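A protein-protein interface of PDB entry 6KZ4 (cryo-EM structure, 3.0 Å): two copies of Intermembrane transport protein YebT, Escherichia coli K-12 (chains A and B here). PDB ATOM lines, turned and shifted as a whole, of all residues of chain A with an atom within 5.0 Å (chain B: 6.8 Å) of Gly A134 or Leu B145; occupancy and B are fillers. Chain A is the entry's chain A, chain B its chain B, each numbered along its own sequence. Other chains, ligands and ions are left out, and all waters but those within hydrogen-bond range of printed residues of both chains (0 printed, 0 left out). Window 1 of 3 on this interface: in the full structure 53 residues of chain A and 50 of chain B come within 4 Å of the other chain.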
ATOM      1  N   PHE A 131     -22.275  21.868   0.594  1.00  0.00           N
ATOM      2  CA  PHE A 131     -20.963  21.780   1.214  1.00  0.00           C
ATOM      3  C   PHE A 131     -20.737  20.463   1.933  1.00  0.00           C
ATOM      4  O   PHE A 131     -19.615  20.197   2.368  1.00  0.00           O
ATOM      5  CB  PHE A 131     -20.769  22.936   2.200  1.00  0.00           C
ATOM      6  CG  PHE A 131     -20.600  24.268   1.540  1.00  0.00           C
ATOM      7  CD1 PHE A 131     -19.730  24.421   0.476  1.00  0.00           C
ATOM      8  CD2 PHE A 131     -21.316  25.367   1.976  1.00  0.00           C
ATOM      9  CE1 PHE A 131     -19.575  25.645  -0.137  1.00  0.00           C
ATOM     10  CE2 PHE A 131     -21.165  26.592   1.368  1.00  0.00           C
ATOM     11  CZ  PHE A 131     -20.293  26.731   0.310  1.00  0.00           C
ATOM     12  N   ASP A 132     -21.771  19.638   2.067  1.00  0.00           N
ATOM     13  CA  ASP A 132     -21.670  18.373   2.784  1.00  0.00           C
ATOM     14  C   ASP A 132     -22.870  17.529   2.395  1.00  0.00           C
ATOM     15  O   ASP A 132     -24.009  17.992   2.501  1.00  0.00           O
ATOM     16  CB  ASP A 132     -21.631  18.607   4.293  1.00  0.00           C
ATOM     17  CG  ASP A 132     -21.542  17.319   5.087  1.00  0.00           C
ATOM     18  OD1 ASP A 132     -20.470  16.681   5.073  1.00  0.00           O
ATOM     19  OD2 ASP A 132     -22.542  16.950   5.739  1.00  0.00           O
ATOM     20  N   ALA A 133     -22.622  16.306   1.936  1.00  0.00           N
ATOM     21  CA  ALA A 133     -23.688  15.405   1.528  1.00  0.00           C
ATOM     22  C   ALA A 133     -24.097  14.445   2.632  1.00  0.00           C
ATOM     23  O   ALA A 133     -24.799  13.467   2.358  1.00  0.00           O
ATOM     24  CB  ALA A 133     -23.267  14.621   0.285  1.00  0.00           C
ATOM     25  N   GLY A 134     -23.670  14.694   3.867  1.00  0.00           N
ATOM     26  CA  GLY A 134     -24.053  13.815   4.955  1.00  0.00           C
ATOM     27  C   GLY A 134     -25.546  13.790   5.188  1.00  0.00           C
ATOM     28  O   GLY A 134     -26.099  12.764   5.591  1.00  0.00           O
ATOM     29  N   LYS A 135     -26.219  14.909   4.939  1.00  0.00           N
ATOM     30  CA  LYS A 135     -27.662  14.980   5.101  1.00  0.00           C
ATOM     31  C   LYS A 135     -28.417  14.487   3.877  1.00  0.00           C
ATOM     32  O   LYS A 135     -29.620  14.227   3.980  1.00  0.00           O
ATOM     33  CB  LYS A 135     -28.086  16.415   5.408  1.00  0.00           C
ATOM     34  CG  LYS A 135     -27.259  17.102   6.472  1.00  0.00           C
ATOM     35  CD  LYS A 135     -27.587  16.574   7.851  1.00  0.00           C
ATOM     36  CE  LYS A 135     -26.910  17.404   8.924  1.00  0.00           C
ATOM     37  NZ  LYS A 135     -27.339  18.826   8.859  1.00  0.00           N
ATOM     38  N   LEU A 136     -27.753  14.347   2.737  1.00  0.00           N
ATOM     39  CA  LEU A 136     -28.402  14.025   1.477  1.00  0.00           C
ATOM     40  C   LEU A 136     -28.323  12.533   1.179  1.00  0.00           C
ATOM     41  O   LEU A 136     -27.490  11.805   1.723  1.00  0.00           O
ATOM     42  CB  LEU A 136     -27.770  14.808   0.325  1.00  0.00           C
ATOM     43  CG  LEU A 136     -28.151  16.276   0.166  1.00  0.00           C
ATOM     44  CD1 LEU A 136     -27.439  17.117   1.189  1.00  0.00           C
ATOM     45  CD2 LEU A 136     -27.815  16.747  -1.224  1.00  0.00           C
ATOM     46  N   LEU A 157     -19.083  14.053  -6.032  1.00  0.00           N
ATOM     47  CA  LEU A 157     -18.116  14.772  -5.210  1.00  0.00           C
ATOM     48  C   LEU A 157     -17.117  15.444  -6.141  1.00  0.00           C
ATOM     49  O   LEU A 157     -16.219  14.792  -6.680  1.00  0.00           O
ATOM     50  CB  LEU A 157     -17.418  13.833  -4.233  1.00  0.00           C
ATOM     51  CG  LEU A 157     -16.159  14.363  -3.548  1.00  0.00           C
ATOM     52  CD1 LEU A 157     -16.440  15.666  -2.836  1.00  0.00           C
ATOM     53  CD2 LEU A 157     -15.615  13.338  -2.579  1.00  0.00           C
ATOM     54  N   ASN A 162     -14.412  22.254  -3.686  1.00  0.00           N
ATOM     55  CA  ASN A 162     -14.638  21.308  -2.603  1.00  0.00           C
ATOM     56  C   ASN A 162     -16.098  21.322  -2.175  1.00  0.00           C
ATOM     57  O   ASN A 162     -16.437  21.838  -1.107  1.00  0.00           O
ATOM     58  CB  ASN A 162     -13.734  21.625  -1.415  1.00  0.00           C
ATOM     59  CG  ASN A 162     -12.268  21.620  -1.786  1.00  0.00           C
ATOM     60  OD1 ASN A 162     -11.707  22.649  -2.160  1.00  0.00           O
ATOM     61  ND2 ASN A 162     -11.638  20.456  -1.688  1.00  0.00           N
ATOM     62  N   GLU A 163     -16.962  20.751  -3.009  1.00  0.00           N
ATOM     63  CA  GLU A 163     -18.392  20.737  -2.755  1.00  0.00           C
ATOM     64  C   GLU A 163     -18.998  19.523  -3.437  1.00  0.00           C
ATOM     65  O   GLU A 163     -18.385  18.904  -4.308  1.00  0.00           O
ATOM     66  CB  GLU A 163     -19.060  22.015  -3.259  1.00  0.00           C
ATOM     67  CG  GLU A 163     -19.193  22.074  -4.765  1.00  0.00           C
ATOM     68  CD  GLU A 163     -19.783  23.378  -5.245  1.00  0.00           C
ATOM     69  OE1 GLU A 163     -19.871  24.323  -4.436  1.00  0.00           O
ATOM     70  OE2 GLU A 163     -20.163  23.459  -6.430  1.00  0.00           O
ATOM     71  N   VAL A 164     -20.217  19.192  -3.032  1.00  0.00           N
ATOM     72  CA  VAL A 164     -20.954  18.064  -3.583  1.00  0.00           C
ATOM     73  C   VAL A 164     -22.037  18.614  -4.496  1.00  0.00           C
ATOM     74  O   VAL A 164     -22.833  19.464  -4.084  1.00  0.00           O
ATOM     75  CB  VAL A 164     -21.562  17.197  -2.471  1.00  0.00           C
ATOM     76  CG1 VAL A 164     -22.576  16.240  -3.048  1.00  0.00           C
ATOM     77  CG2 VAL A 164     -20.474  16.445  -1.745  1.00  0.00           C
ATOM     78  N   ARG B 143     -15.214   8.988   4.914  1.00  0.00           N
ATOM     79  CA  ARG B 143     -15.997   9.908   4.106  1.00  0.00           C
ATOM     80  C   ARG B 143     -15.402  11.307   4.115  1.00  0.00           C
ATOM     81  O   ARG B 143     -14.774  11.730   5.087  1.00  0.00           O
ATOM     82  CB  ARG B 143     -17.440   9.968   4.593  1.00  0.00           C
ATOM     83  CG  ARG B 143     -18.151   8.640   4.513  1.00  0.00           C
ATOM     84  CD  ARG B 143     -19.614   8.773   4.840  1.00  0.00           C
ATOM     85  NE  ARG B 143     -20.225   7.465   5.031  1.00  0.00           N
ATOM     86  CZ  ARG B 143     -21.412   7.272   5.592  1.00  0.00           C
ATOM     87  NH1 ARG B 143     -22.115   8.306   6.020  1.00  0.00           N
ATOM     88  NH2 ARG B 143     -21.891   6.045   5.729  1.00  0.00           N
ATOM     89  N   TYR B 144     -15.617  12.019   3.013  1.00  0.00           N
ATOM     90  CA  TYR B 144     -15.244  13.420   2.877  1.00  0.00           C
ATOM     91  C   TYR B 144     -16.427  14.145   2.257  1.00  0.00           C
ATOM     92  O   TYR B 144     -16.834  13.818   1.139  1.00  0.00           O
ATOM     93  CB  TYR B 144     -13.993  13.583   2.021  1.00  0.00           C
ATOM     94  CG  TYR B 144     -13.735  15.000   1.589  1.00  0.00           C
ATOM     95  CD1 TYR B 144     -13.512  15.996   2.520  1.00  0.00           C
ATOM     96  CD2 TYR B 144     -13.709  15.340   0.249  1.00  0.00           C
ATOM     97  CE1 TYR B 144     -13.277  17.290   2.133  1.00  0.00           C
ATOM     98  CE2 TYR B 144     -13.472  16.635  -0.148  1.00  0.00           C
ATOM     99  CZ  TYR B 144     -13.257  17.605   0.799  1.00  0.00           C
ATOM    100  OH  TYR B 144     -13.018  18.900   0.411  1.00  0.00           O
ATOM    101  N   LEU B 145     -16.984  15.107   2.988  1.00  0.00           N
ATOM    102  CA  LEU B 145     -18.182  15.839   2.588  1.00  0.00           C
ATOM    103  C   LEU B 145     -19.395  14.931   2.453  1.00  0.00           C
ATOM    104  O   LEU B 145     -20.409  15.331   1.878  1.00  0.00           O
ATOM    105  CB  LEU B 145     -17.962  16.613   1.286  1.00  0.00           C
ATOM    106  CG  LEU B 145     -16.789  17.583   1.273  1.00  0.00           C
ATOM    107  CD1 LEU B 145     -16.766  18.364  -0.020  1.00  0.00           C
ATOM    108  CD2 LEU B 145     -16.889  18.507   2.457  1.00  0.00           C
ATOM    109  N   GLY B 146     -19.317  13.711   2.971  1.00  0.00           N
ATOM    110  CA  GLY B 146     -20.414  12.774   2.909  1.00  0.00           C
ATOM    111  C   GLY B 146     -20.286  11.713   1.840  1.00  0.00           C
ATOM    112  O   GLY B 146     -21.147  10.832   1.762  1.00  0.00           O
ATOM    113  N   ILE B 147     -19.250  11.773   1.018  1.00  0.00           N
ATOM    114  CA  ILE B 147     -19.020  10.782  -0.024  1.00  0.00           C
ATOM    115  C   ILE B 147     -17.911   9.851   0.438  1.00  0.00           C
ATOM    116  O   ILE B 147     -16.918  10.300   1.019  1.00  0.00           O
ATOM    117  CB  ILE B 147     -18.657  11.461  -1.352  1.00  0.00           C
ATOM    118  CG1 ILE B 147     -19.557  12.673  -1.588  1.00  0.00           C
ATOM    119  CG2 ILE B 147     -18.788  10.487  -2.497  1.00  0.00           C
ATOM    120  CD1 ILE B 147     -21.017  12.331  -1.679  1.00  0.00           C
ATOM    121  N   ILE B 149     -14.698   7.785   0.636  1.00  0.00           N
ATOM    122  CA  ILE B 149     -13.373   7.987   0.064  1.00  0.00           C
ATOM    123  C   ILE B 149     -12.588   6.691   0.197  1.00  0.00           C
ATOM    124  O   ILE B 149     -11.707   6.394  -0.615  1.00  0.00           O
ATOM    125  CB  ILE B 149     -12.658   9.159   0.759  1.00  0.00           C
ATOM    126  CG1 ILE B 149     -13.405  10.457   0.489  1.00  0.00           C
ATOM    127  CG2 ILE B 149     -11.234   9.289   0.291  1.00  0.00           C
ATOM    128  CD1 ILE B 149     -13.871  10.601  -0.930  1.00  0.00           C
ATOM    129  N   ASP B 201     -27.573   9.417  12.439  1.00  0.00           N
ATOM    130  CA  ASP B 201     -27.362   8.328  11.497  1.00  0.00           C
ATOM    131  C   ASP B 201     -26.128   7.511  11.839  1.00  0.00           C
ATOM    132  O   ASP B 201     -25.968   6.403  11.318  1.00  0.00           O
ATOM    133  CB  ASP B 201     -27.265   8.880  10.077  1.00  0.00           C
ATOM    134  CG  ASP B 201     -26.295  10.039   9.967  1.00  0.00           C
ATOM    135  OD1 ASP B 201     -25.102   9.856  10.282  1.00  0.00           O
ATOM    136  OD2 ASP B 201     -26.730  11.137   9.564  1.00  0.00           O
ATOM    137  N   TYR B 207     -18.932   6.306  10.932  1.00  0.00           N
ATOM    138  CA  TYR B 207     -17.938   6.480   9.887  1.00  0.00           C
ATOM    139  C   TYR B 207     -16.825   7.393  10.374  1.00  0.00           C
ATOM    140  O   TYR B 207     -16.893   7.976  11.456  1.00  0.00           O
ATOM    141  CB  TYR B 207     -18.566   7.047   8.614  1.00  0.00           C
ATOM    142  CG  TYR B 207     -19.092   8.452   8.760  1.00  0.00           C
ATOM    143  CD1 TYR B 207     -20.305   8.702   9.374  1.00  0.00           C
ATOM    144  CD2 TYR B 207     -18.376   9.531   8.271  1.00  0.00           C
ATOM    145  CE1 TYR B 207     -20.784   9.982   9.501  1.00  0.00           C
ATOM    146  CE2 TYR B 207     -18.848  10.813   8.400  1.00  0.00           C
ATOM    147  CZ  TYR B 207     -20.053  11.033   9.013  1.00  0.00           C
ATOM    148  OH  TYR B 207     -20.529  12.314   9.138  1.00  0.00           O
ATOM    149  N   ASN B 209     -14.530  10.754   9.419  1.00  0.00           N
ATOM    150  CA  ASN B 209     -14.542  11.979   8.635  1.00  0.00           C
ATOM    151  C   ASN B 209     -13.119  12.440   8.358  1.00  0.00           C
ATOM    152  O   ASN B 209     -12.207  12.210   9.155  1.00  0.00           O
ATOM    153  CB  ASN B 209     -15.313  13.073   9.367  1.00  0.00           C
ATOM    154  CG  ASN B 209     -15.465  14.322   8.543  1.00  0.00           C
ATOM    155  OD1 ASN B 209     -15.502  14.270   7.317  1.00  0.00           O
ATOM    156  ND2 ASN B 209     -15.548  15.461   9.212  1.00  0.00           N
ATOM    157  N   VAL B 210     -12.935  13.096   7.214  1.00  0.00           N
ATOM    158  CA  VAL B 210     -11.615  13.465   6.718  1.00  0.00           C
ATOM    159  C   VAL B 210     -11.592  14.947   6.388  1.00  0.00           C
ATOM    160  O   VAL B 210     -12.602  15.514   5.961  1.00  0.00           O
ATOM    161  CB  VAL B 210     -11.233  12.636   5.479  1.00  0.00           C
ATOM    162  CG1 VAL B 210      -9.773  12.810   5.152  1.00  0.00           C
ATOM    163  CG2 VAL B 210     -11.532  11.196   5.716  1.00  0.00           C
ATOM    164  N   ILE B 228     -13.287  19.351  11.311  1.00  0.00           N
ATOM    165  CA  ILE B 228     -14.268  20.199  10.646  1.00  0.00           C
ATOM    166  C   ILE B 228     -15.049  19.342   9.662  1.00  0.00           C
ATOM    167  O   ILE B 228     -14.470  18.703   8.777  1.00  0.00           O
ATOM    168  CB  ILE B 228     -13.590  21.383   9.950  1.00  0.00           C
ATOM    169  CG1 ILE B 228     -12.727  22.150  10.948  1.00  0.00           C
ATOM    170  CG2 ILE B 228     -14.629  22.306   9.355  1.00  0.00           C
ATOM    171  CD1 ILE B 228     -13.506  22.698  12.114  1.00  0.00           C
ATOM    172  N   THR B 229     -16.372  19.316   9.819  1.00  0.00           N
ATOM    173  CA  THR B 229     -17.197  18.403   9.036  1.00  0.00           C
ATOM    174  C   THR B 229     -17.270  18.835   7.576  1.00  0.00           C
ATOM    175  O   THR B 229     -16.937  18.063   6.670  1.00  0.00           O
ATOM    176  CB  THR B 229     -18.597  18.313   9.645  1.00  0.00           C
ATOM    177  OG1 THR B 229     -19.085  19.629   9.925  1.00  0.00           O
ATOM    178  CG2 THR B 229     -18.561  17.508  10.931  1.00  0.00           C
ATOM    179  N   ASP B 230     -17.706  20.062   7.329  1.00  0.00           N
ATOM    180  CA  ASP B 230     -17.901  20.566   5.980  1.00  0.00           C
ATOM    181  C   ASP B 230     -16.712  21.407   5.539  1.00  0.00           C
ATOM    182  O   ASP B 230     -15.957  21.943   6.354  1.00  0.00           O
ATOM    183  CB  ASP B 230     -19.183  21.391   5.898  1.00  0.00           C
ATOM    184  CG  ASP B 230     -19.169  22.578   6.838  1.00  0.00           C
ATOM    185  OD1 ASP B 230     -19.687  23.646   6.456  1.00  0.00           O
ATOM    186  OD2 ASP B 230     -18.632  22.445   7.957  1.00  0.00           O
ATOM    187  N   SER B 231     -16.557  21.523   4.221  1.00  0.00           N
ATOM    188  CA  SER B 231     -15.469  22.285   3.622  1.00  0.00           C
ATOM    189  C   SER B 231     -15.859  23.722   3.320  1.00  0.00           C
ATOM    190  O   SER B 231     -15.325  24.321   2.378  1.00  0.00           O
ATOM    191  CB  SER B 231     -14.983  21.592   2.350  1.00  0.00           C
ATOM    192  OG  SER B 231     -13.950  22.337   1.735  1.00  0.00           O
ATOM    193  N   ARG B 232     -16.784  24.290   4.094  1.00  0.00           N
ATOM    194  CA  ARG B 232     -17.216  25.661   3.851  1.00  0.00           C
ATOM    195  C   ARG B 232     -16.069  26.643   4.045  1.00  0.00           C
ATOM    196  O   ARG B 232     -15.997  27.669   3.360  1.00  0.00           O
ATOM    197  CB  ARG B 232     -18.382  26.007   4.774  1.00  0.00           C
ATOM    198  CG  ARG B 232     -19.043  27.328   4.473  1.00  0.00           C
ATOM    199  CD  ARG B 232     -20.112  27.658   5.499  1.00  0.00           C
ATOM    200  NE  ARG B 232     -21.343  26.912   5.269  1.00  0.00           N
ATOM    201  CZ  ARG B 232     -21.732  25.876   6.002  1.00  0.00           C
ATOM    202  NH1 ARG B 232     -20.982  25.463   7.013  1.00  0.00           N
ATOM    203  NH2 ARG B 232     -22.869  25.253   5.724  1.00  0.00           N
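Printed residues of chain B within 4 Å of Phe A131: Leu B145 (3.2 Å), Asp B230 (3.8 Å), Ser B231 (3.8 Å) and Arg B232 (3.6 Å).
Of the printed residues of chain B, Asp A132 touches Leu B145 (3.3 Å) and Gly B146 (3.8 Å).
Of chain B, only Leu B145 (3.9 Å) and Gly B146 (3.9 Å) come within 4 Å of Gly A134.
Lys A135 touches none of the printed residues of chain B.
Of the printed residues of chain A, Tyr B144 touches Leu A157 and Asn A162.
Leu B145 touches eight residues of chain A.
Of the printed residues of chain A, Ile B147 touches Ala A133, Leu A157 and Val A164.
Of the printed residues of chain A, Arg B232 touches Phe A131 (3.6 Å).
The nearest residue of chain B that does not touch Gly A134 is Asp B201 (4.3 Å).
No position is printed for both chains.
Of the 20 pairs that touch across the chains among the printed residues, none has its exchanged pair printed and touching as well.
Printed residues of chain B that touch a printed residue of chain A: Tyr B144, Leu B145, Gly B146, Ile B147, Ile B149, Asp B230, Ser B231 and Arg B232.
Hydrophobic or aromatic side chains of chain B that line the printed part of chain A: Tyr B144, Leu B145, Ile B147 and Ile B149.
Of the 10 printed residues of chain A, 8 touch a printed residue of chain B.
Hydrophobic or aromatic side chains of chain A within 4 Å of the printed part of chain B: Phe A131, Ala A133, Leu A157 and Val A164.
Ser B231 touches Phe A131.
NE of Arg B232 touches CD2 of Phe A131 (3.6 Å).
CB of Ala A133 touches CD1 of Ile B147, at 3.8 Å.
N of Gly A134 touches O of Leu B145 (3.9 Å).
Leu B145 touches Leu A157.
Leu A157 touches Ile B147 (CB to CG1, 3.6 Å).
Leu A157 touches Ile B149 (CD2 to CD1, 3.6 Å).
CD1 of Leu B145 touches O of Asn A162 (3.7 Å).
CG2 of Val A164 touches O of Leu B145 (3.8 Å).
CG2 of Val A164 touches CG1 of Ile B147, 3.9 Å away.
N of Gly A134 is in hydrogen-bond range of OD2 of Asp A132, 3.1 Å away.
The side-chain carboxylate (OD2) of Asp B230 lies within hydrogen-bond range of the side-chain hydroxyl (OG1) of Thr B229 (3.5 Å).
OD1 of Asp B230 lies within salt-bridge range of NH2 of Arg B232 (3.6 Å).
The backbone NH (N) of Ala A133 lies within hydrogen-bond range of the backbone carbonyl oxygen (O) of Leu B145, 2.4 Å away.
The side-chain hydroxyl (OH) of Tyr B144 sits at hydrogen-bond distance from the side-chain amide nitrogen (ND2) of Asn A162.
The side-chain carboxylate of Asp A132 lies close to the backbone carbonyl oxygen of Leu B145 (3.5 Å).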
